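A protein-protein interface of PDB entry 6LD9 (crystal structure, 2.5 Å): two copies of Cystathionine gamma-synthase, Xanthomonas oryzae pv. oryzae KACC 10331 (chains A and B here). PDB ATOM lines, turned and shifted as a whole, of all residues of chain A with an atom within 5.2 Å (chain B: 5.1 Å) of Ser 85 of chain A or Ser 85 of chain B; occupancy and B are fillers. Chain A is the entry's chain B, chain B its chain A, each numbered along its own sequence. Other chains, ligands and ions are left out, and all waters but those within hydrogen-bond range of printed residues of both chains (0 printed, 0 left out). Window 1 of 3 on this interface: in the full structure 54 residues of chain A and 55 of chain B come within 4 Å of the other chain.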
ATOM      1  N   ILE A  83      -2.803 -18.333 -23.959  1.00  0.00           N
ATOM      2  CA  ILE A  83      -1.558 -18.416 -23.186  1.00  0.00           C
ATOM      3  C   ILE A  83      -0.378 -18.315 -24.140  1.00  0.00           C
ATOM      4  O   ILE A  83      -0.274 -19.113 -25.042  1.00  0.00           O
ATOM      5  CB  ILE A  83      -1.560 -19.729 -22.407  1.00  0.00           C
ATOM      6  CG1 ILE A  83      -2.831 -19.911 -21.585  1.00  0.00           C
ATOM      7  CG2 ILE A  83      -0.321 -19.831 -21.531  1.00  0.00           C
ATOM      8  CD1 ILE A  83      -3.123 -18.761 -20.664  1.00  0.00           C
ATOM      9  N   THR A  84       0.531 -17.388 -23.909  1.00  0.00           N
ATOM     10  CA  THR A  84       1.693 -17.124 -24.799  1.00  0.00           C
ATOM     11  C   THR A  84       2.968 -17.589 -24.090  1.00  0.00           C
ATOM     12  O   THR A  84       2.908 -17.738 -22.868  1.00  0.00           O
ATOM     13  CB  THR A  84       1.729 -15.634 -25.159  1.00  0.00           C
ATOM     14  OG1 THR A  84       1.739 -14.825 -23.976  1.00  0.00           O
ATOM     15  CG2 THR A  84       0.522 -15.252 -25.988  1.00  0.00           C
ATOM     16  N   SER A  85       4.064 -17.786 -24.812  1.00  0.00           N
ATOM     17  CA  SER A  85       5.393 -18.156 -24.258  1.00  0.00           C
ATOM     18  C   SER A  85       5.846 -17.104 -23.242  1.00  0.00           C
ATOM     19  O   SER A  85       6.575 -17.470 -22.301  1.00  0.00           O
ATOM     20  CB  SER A  85       6.413 -18.257 -25.328  1.00  0.00           C
ATOM     21  OG  SER A  85       6.191 -17.158 -26.213  1.00  0.00           O
ATOM     22  N   THR A  86       5.518 -15.835 -23.451  1.00  0.00           N
ATOM     23  CA  THR A  86       5.931 -14.763 -22.519  1.00  0.00           C
ATOM     24  C   THR A  86       4.854 -13.674 -22.452  1.00  0.00           C
ATOM     25  O   THR A  86       3.929 -13.684 -23.295  1.00  0.00           O
ATOM     26  CB  THR A  86       7.275 -14.120 -22.906  1.00  0.00           C
ATOM     27  OG1 THR A  86       7.066 -13.275 -24.036  1.00  0.00           O
ATOM     28  CG2 THR A  86       8.399 -15.106 -23.189  1.00  0.00           C
ATOM     29  N   GLY A  87       4.987 -12.787 -21.456  1.00  0.00           N
ATOM     30  CA  GLY A  87       4.212 -11.554 -21.332  1.00  0.00           C
ATOM     31  C   GLY A  87       4.436 -10.607 -22.509  1.00  0.00           C
ATOM     32  O   GLY A  87       3.434 -10.069 -23.037  1.00  0.00           O
ATOM     33  N   VAL A 218       8.287 -18.291 -17.349  1.00  0.00           N
ATOM     34  CA  VAL A 218       8.002 -17.033 -18.059  1.00  0.00           C
ATOM     35  C   VAL A 218       6.828 -17.389 -18.946  1.00  0.00           C
ATOM     36  O   VAL A 218       6.889 -18.448 -19.634  1.00  0.00           O
ATOM     37  CB  VAL A 218       9.223 -16.591 -18.853  1.00  0.00           C
ATOM     38  CG1 VAL A 218       8.912 -15.408 -19.703  1.00  0.00           C
ATOM     39  CG2 VAL A 218      10.352 -16.232 -17.954  1.00  0.00           C
ATOM     40  N   GLY A 219       5.794 -16.558 -18.924  1.00  0.00           N
ATOM     41  CA  GLY A 219       4.554 -16.738 -19.702  1.00  0.00           C
ATOM     42  C   GLY A 219       3.666 -15.506 -19.753  1.00  0.00           C
ATOM     43  O   GLY A 219       3.858 -14.525 -18.961  1.00  0.00           O
ATOM     44  N   GLY A 220       2.695 -15.547 -20.662  1.00  0.00           N
ATOM     45  CA  GLY A 220       1.709 -14.462 -20.795  1.00  0.00           C
ATOM     46  C   GLY A 220       0.319 -15.020 -20.999  1.00  0.00           C
ATOM     47  O   GLY A 220       0.212 -16.201 -21.303  1.00  0.00           O
ATOM     48  N   GLY A 241       2.873 -18.353 -34.039  1.00  0.00           N
ATOM     49  CA  GLY A 241       3.671 -19.299 -33.242  1.00  0.00           C
ATOM     50  C   GLY A 241       4.023 -18.760 -31.853  1.00  0.00           C
ATOM     51  O   GLY A 241       5.120 -19.111 -31.384  1.00  0.00           O
ATOM     52  N   LEU A 242       3.125 -17.963 -31.254  1.00  0.00           N
ATOM     53  CA  LEU A 242       3.303 -17.254 -29.955  1.00  0.00           C
ATOM     54  C   LEU A 242       2.816 -18.119 -28.783  1.00  0.00           C
ATOM     55  O   LEU A 242       3.052 -17.697 -27.678  1.00  0.00           O
ATOM     56  CB  LEU A 242       2.534 -15.922 -29.963  1.00  0.00           C
ATOM     57  CG  LEU A 242       3.163 -14.835 -30.817  1.00  0.00           C
ATOM     58  CD1 LEU A 242       2.248 -13.647 -30.881  1.00  0.00           C
ATOM     59  CD2 LEU A 242       4.518 -14.370 -30.282  1.00  0.00           C
ATOM     60  N   THR A 243       2.192 -19.268 -28.997  1.00  0.00           N
ATOM     61  CA  THR A 243       1.613 -20.087 -27.897  1.00  0.00           C
ATOM     62  C   THR A 243       2.699 -20.644 -26.992  1.00  0.00           C
ATOM     63  O   THR A 243       3.805 -20.764 -27.446  1.00  0.00           O
ATOM     64  CB  THR A 243       0.708 -21.203 -28.428  1.00  0.00           C
ATOM     65  OG1 THR A 243       1.363 -21.924 -29.474  1.00  0.00           O
ATOM     66  CG2 THR A 243      -0.585 -20.596 -28.931  1.00  0.00           C
ATOM     67  N   GLY A 244       2.360 -20.825 -25.700  1.00  0.00           N
ATOM     68  CA  GLY A 244       3.246 -21.320 -24.632  1.00  0.00           C
ATOM     69  C   GLY A 244       3.322 -22.838 -24.574  1.00  0.00           C
ATOM     70  O   GLY A 244       2.496 -23.543 -25.159  1.00  0.00           O
ATOM     71  N   ILE B  83      16.350 -20.075 -29.654  1.00  0.00           N
ATOM     72  CA  ILE B  83      15.325 -21.114 -29.474  1.00  0.00           C
ATOM     73  C   ILE B  83      14.014 -20.403 -29.234  1.00  0.00           C
ATOM     74  O   ILE B  83      13.973 -19.598 -28.301  1.00  0.00           O
ATOM     75  CB  ILE B  83      15.699 -22.017 -28.300  1.00  0.00           C
ATOM     76  CG1 ILE B  83      17.089 -22.598 -28.481  1.00  0.00           C
ATOM     77  CG2 ILE B  83      14.702 -23.115 -28.122  1.00  0.00           C
ATOM     78  CD1 ILE B  83      17.320 -23.226 -29.803  1.00  0.00           C
ATOM     79  N   THR B  84      12.987 -20.696 -30.038  1.00  0.00           N
ATOM     80  CA  THR B  84      11.655 -20.029 -29.975  1.00  0.00           C
ATOM     81  C   THR B  84      10.615 -21.014 -29.429  1.00  0.00           C
ATOM     82  O   THR B  84      10.938 -22.177 -29.300  1.00  0.00           O
ATOM     83  CB  THR B  84      11.309 -19.486 -31.356  1.00  0.00           C
ATOM     84  OG1 THR B  84      11.349 -20.572 -32.265  1.00  0.00           O
ATOM     85  CG2 THR B  84      12.306 -18.451 -31.825  1.00  0.00           C
ATOM     86  N   SER B  85       9.456 -20.541 -29.029  1.00  0.00           N
ATOM     87  CA  SER B  85       8.351 -21.368 -28.477  1.00  0.00           C
ATOM     88  C   SER B  85       7.842 -22.347 -29.549  1.00  0.00           C
ATOM     89  O   SER B  85       7.322 -23.436 -29.154  1.00  0.00           O
ATOM     90  CB  SER B  85       7.241 -20.496 -27.998  1.00  0.00           C
ATOM     91  OG  SER B  85       7.182 -19.374 -28.901  1.00  0.00           O
ATOM     92  N   THR B  86       7.903 -21.979 -30.832  1.00  0.00           N
ATOM     93  CA  THR B  86       7.413 -22.841 -31.935  1.00  0.00           C
ATOM     94  C   THR B  86       8.286 -22.630 -33.162  1.00  0.00           C
ATOM     95  O   THR B  86       9.039 -21.690 -33.161  1.00  0.00           O
ATOM     96  CB  THR B  86       5.957 -22.555 -32.306  1.00  0.00           C
ATOM     97  OG1 THR B  86       5.957 -21.269 -32.945  1.00  0.00           O
ATOM     98  CG2 THR B  86       5.000 -22.592 -31.121  1.00  0.00           C
ATOM     99  N   GLY B  87       8.179 -23.520 -34.144  1.00  0.00           N
ATOM    100  CA  GLY B  87       8.718 -23.360 -35.497  1.00  0.00           C
ATOM    101  C   GLY B  87       8.152 -22.138 -36.212  1.00  0.00           C
ATOM    102  O   GLY B  87       8.971 -21.377 -36.835  1.00  0.00           O
ATOM    103  N   VAL B 218       6.718 -28.667 -28.761  1.00  0.00           N
ATOM    104  CA  VAL B 218       6.659 -27.754 -29.924  1.00  0.00           C
ATOM    105  C   VAL B 218       7.713 -26.708 -29.652  1.00  0.00           C
ATOM    106  O   VAL B 218       7.754 -26.234 -28.535  1.00  0.00           O
ATOM    107  CB  VAL B 218       5.256 -27.164 -30.074  1.00  0.00           C
ATOM    108  CG1 VAL B 218       5.230 -26.119 -31.149  1.00  0.00           C
ATOM    109  CG2 VAL B 218       4.238 -28.223 -30.405  1.00  0.00           C
ATOM    110  N   GLY B 219       8.632 -26.474 -30.587  1.00  0.00           N
ATOM    111  CA  GLY B 219       9.713 -25.458 -30.518  1.00  0.00           C
ATOM    112  C   GLY B 219      10.318 -25.101 -31.867  1.00  0.00           C
ATOM    113  O   GLY B 219      10.040 -25.768 -32.919  1.00  0.00           O
ATOM    114  N   GLY B 220      11.157 -24.070 -31.859  1.00  0.00           N
ATOM    115  CA  GLY B 220      11.844 -23.583 -33.063  1.00  0.00           C
ATOM    116  C   GLY B 220      13.274 -23.201 -32.772  1.00  0.00           C
ATOM    117  O   GLY B 220      13.610 -23.094 -31.613  1.00  0.00           O
ATOM    118  N   GLY B 241       9.273 -11.324 -27.319  1.00  0.00           N
ATOM    119  CA  GLY B 241       8.839 -12.364 -26.364  1.00  0.00           C
ATOM    120  C   GLY B 241       8.619 -13.732 -27.004  1.00  0.00           C
ATOM    121  O   GLY B 241       7.628 -14.382 -26.653  1.00  0.00           O
ATOM    122  N   LEU B 242       9.468 -14.092 -27.965  1.00  0.00           N
ATOM    123  CA  LEU B 242       9.298 -15.277 -28.845  1.00  0.00           C
ATOM    124  C   LEU B 242      10.110 -16.447 -28.288  1.00  0.00           C
ATOM    125  O   LEU B 242      10.035 -17.478 -28.864  1.00  0.00           O
ATOM    126  CB  LEU B 242       9.781 -14.943 -30.268  1.00  0.00           C
ATOM    127  CG  LEU B 242       8.768 -14.176 -31.100  1.00  0.00           C
ATOM    128  CD1 LEU B 242       9.379 -13.764 -32.422  1.00  0.00           C
ATOM    129  CD2 LEU B 242       7.544 -15.018 -31.372  1.00  0.00           C
ATOM    130  N   THR B 243      10.844 -16.273 -27.208  1.00  0.00           N
ATOM    131  CA  THR B 243      11.750 -17.291 -26.627  1.00  0.00           C
ATOM    132  C   THR B 243      10.980 -18.466 -26.037  1.00  0.00           C
ATOM    133  O   THR B 243       9.853 -18.313 -25.571  1.00  0.00           O
ATOM    134  CB  THR B 243      12.730 -16.661 -25.626  1.00  0.00           C
ATOM    135  OG1 THR B 243      12.148 -15.692 -24.735  1.00  0.00           O
ATOM    136  CG2 THR B 243      13.862 -16.014 -26.406  1.00  0.00           C
ATOM    137  N   GLY B 244      11.612 -19.646 -26.137  1.00  0.00           N
ATOM    138  CA  GLY B 244      11.096 -20.922 -25.613  1.00  0.00           C
ATOM    139  C   GLY B 244      11.222 -21.107 -24.102  1.00  0.00           C
ATOM    140  O   GLY B 244      12.067 -20.443 -23.453  1.00  0.00           O
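Ser 85 of chain A touches three residues of chain B.
Of chain A, only Ser 85, Gly 241 and Thr 243 come within 4 Å of Ser 85 of chain B.
Printed residues of chain B within 4 Å of Thr 243 of chain A: Ser 85.
Of the printed residues of chain B, Gly 241 of chain A touches Ser 85 and Thr 86.
Gly 87 of chain B touches none of the printed residues of chain A.
Gly 219 of chain B touches none of the printed residues of chain A.
The nearest residue of chain A that does not touch Ser 85 of chain B is Leu 242 of chain A (4.5 Å).
The nearest printed residue of chain B that does not touch Leu 242 of chain A is Ser 85 of chain B (4.5 Å).
Ser 85 of chain A touches Ser 85 of chain B (CB to CB, 3.6 Å).
CB of Ser 85 of chain A touches O of Thr 243 of chain B, at 3.4 Å.
CD2 of Leu 242 of chain B touches CD2 of Leu 242 of chain A (3.3 Å).
O of Thr 243 of chain A touches CB of Ser 85 of chain B, at 3.5 Å.
Along chain A the printed residues that touch a printed residue of chain B span positions 85 to 243.
Of the 12 printed residues of chain B, 5 touch a printed residue of chain A.
Hydrophobic or aromatic side chains of chain B that line the printed part of chain A: Leu 242.
Among the printed residues, no Asp or Glu carboxylate lies within 4 Å of a Lys or Arg side-chain nitrogen of the other chain.
OG of Ser 85 of chain B is in hydrogen-bond range of O of Gly 241 of chain A, at 3.2 Å.
The backbone carbonyl oxygen (O) of Gly 241 of chain A sits at hydrogen-bond distance from the side-chain hydroxyl (OG1) of Thr 86 of chain B (2.8 Å).
The backbone carbonyl oxygen of Gly 241 of chain B lies within hydrogen-bond range of the side-chain hydroxyl of Ser 85 of chain A (3.2 Å).
The backbone carbonyl oxygen (O) of Gly 241 of chain B sits at hydrogen-bond distance from the side-chain hydroxyl (OG1) of Thr 86 of chain A (2.9 Å).
The backbone carbonyl oxygen of Thr 86 of chain B sits at hydrogen-bond distance from the side-chain hydroxyl of Thr 84 of chain B (2.7 Å).
N of Ser 85 of chain B lies within hydrogen-bond range of O of Leu 242 of chain B (3.1 Å).
The backbone carbonyl oxygen of Thr 86 of chain B lies close to the backbone NH of Gly 220 of chain B (3.4 Å).
OG1 of Thr 84 of chain A lies within hydrogen-bond range of O of Thr 86 of chain A (2.6 Å).
The backbone NH of Ser 85 of chain A is in hydrogen-bond range of the backbone carbonyl oxygen of Leu 242 of chain A (3.0 Å).
O of Thr 86 of chain A lies close to N of Gly 220 of chain A.
Ser 85 of chain A touches Gly 241 of chain B, and with the chains exchanged Gly 241 of chain A touches Ser 85 of chain B.
Ser 85 of chain A touches Thr 243 of chain B, and with the chains exchanged Thr 243 of chain A touches Ser 85 of chain B.
Thr 86 of chain A touches Gly 241 of chain B, and with the chains exchanged Gly 241 of chain A touches Thr 86 of chain B.
Leu 242 of chain A touches its own counterpart, Leu 242 of chain B.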
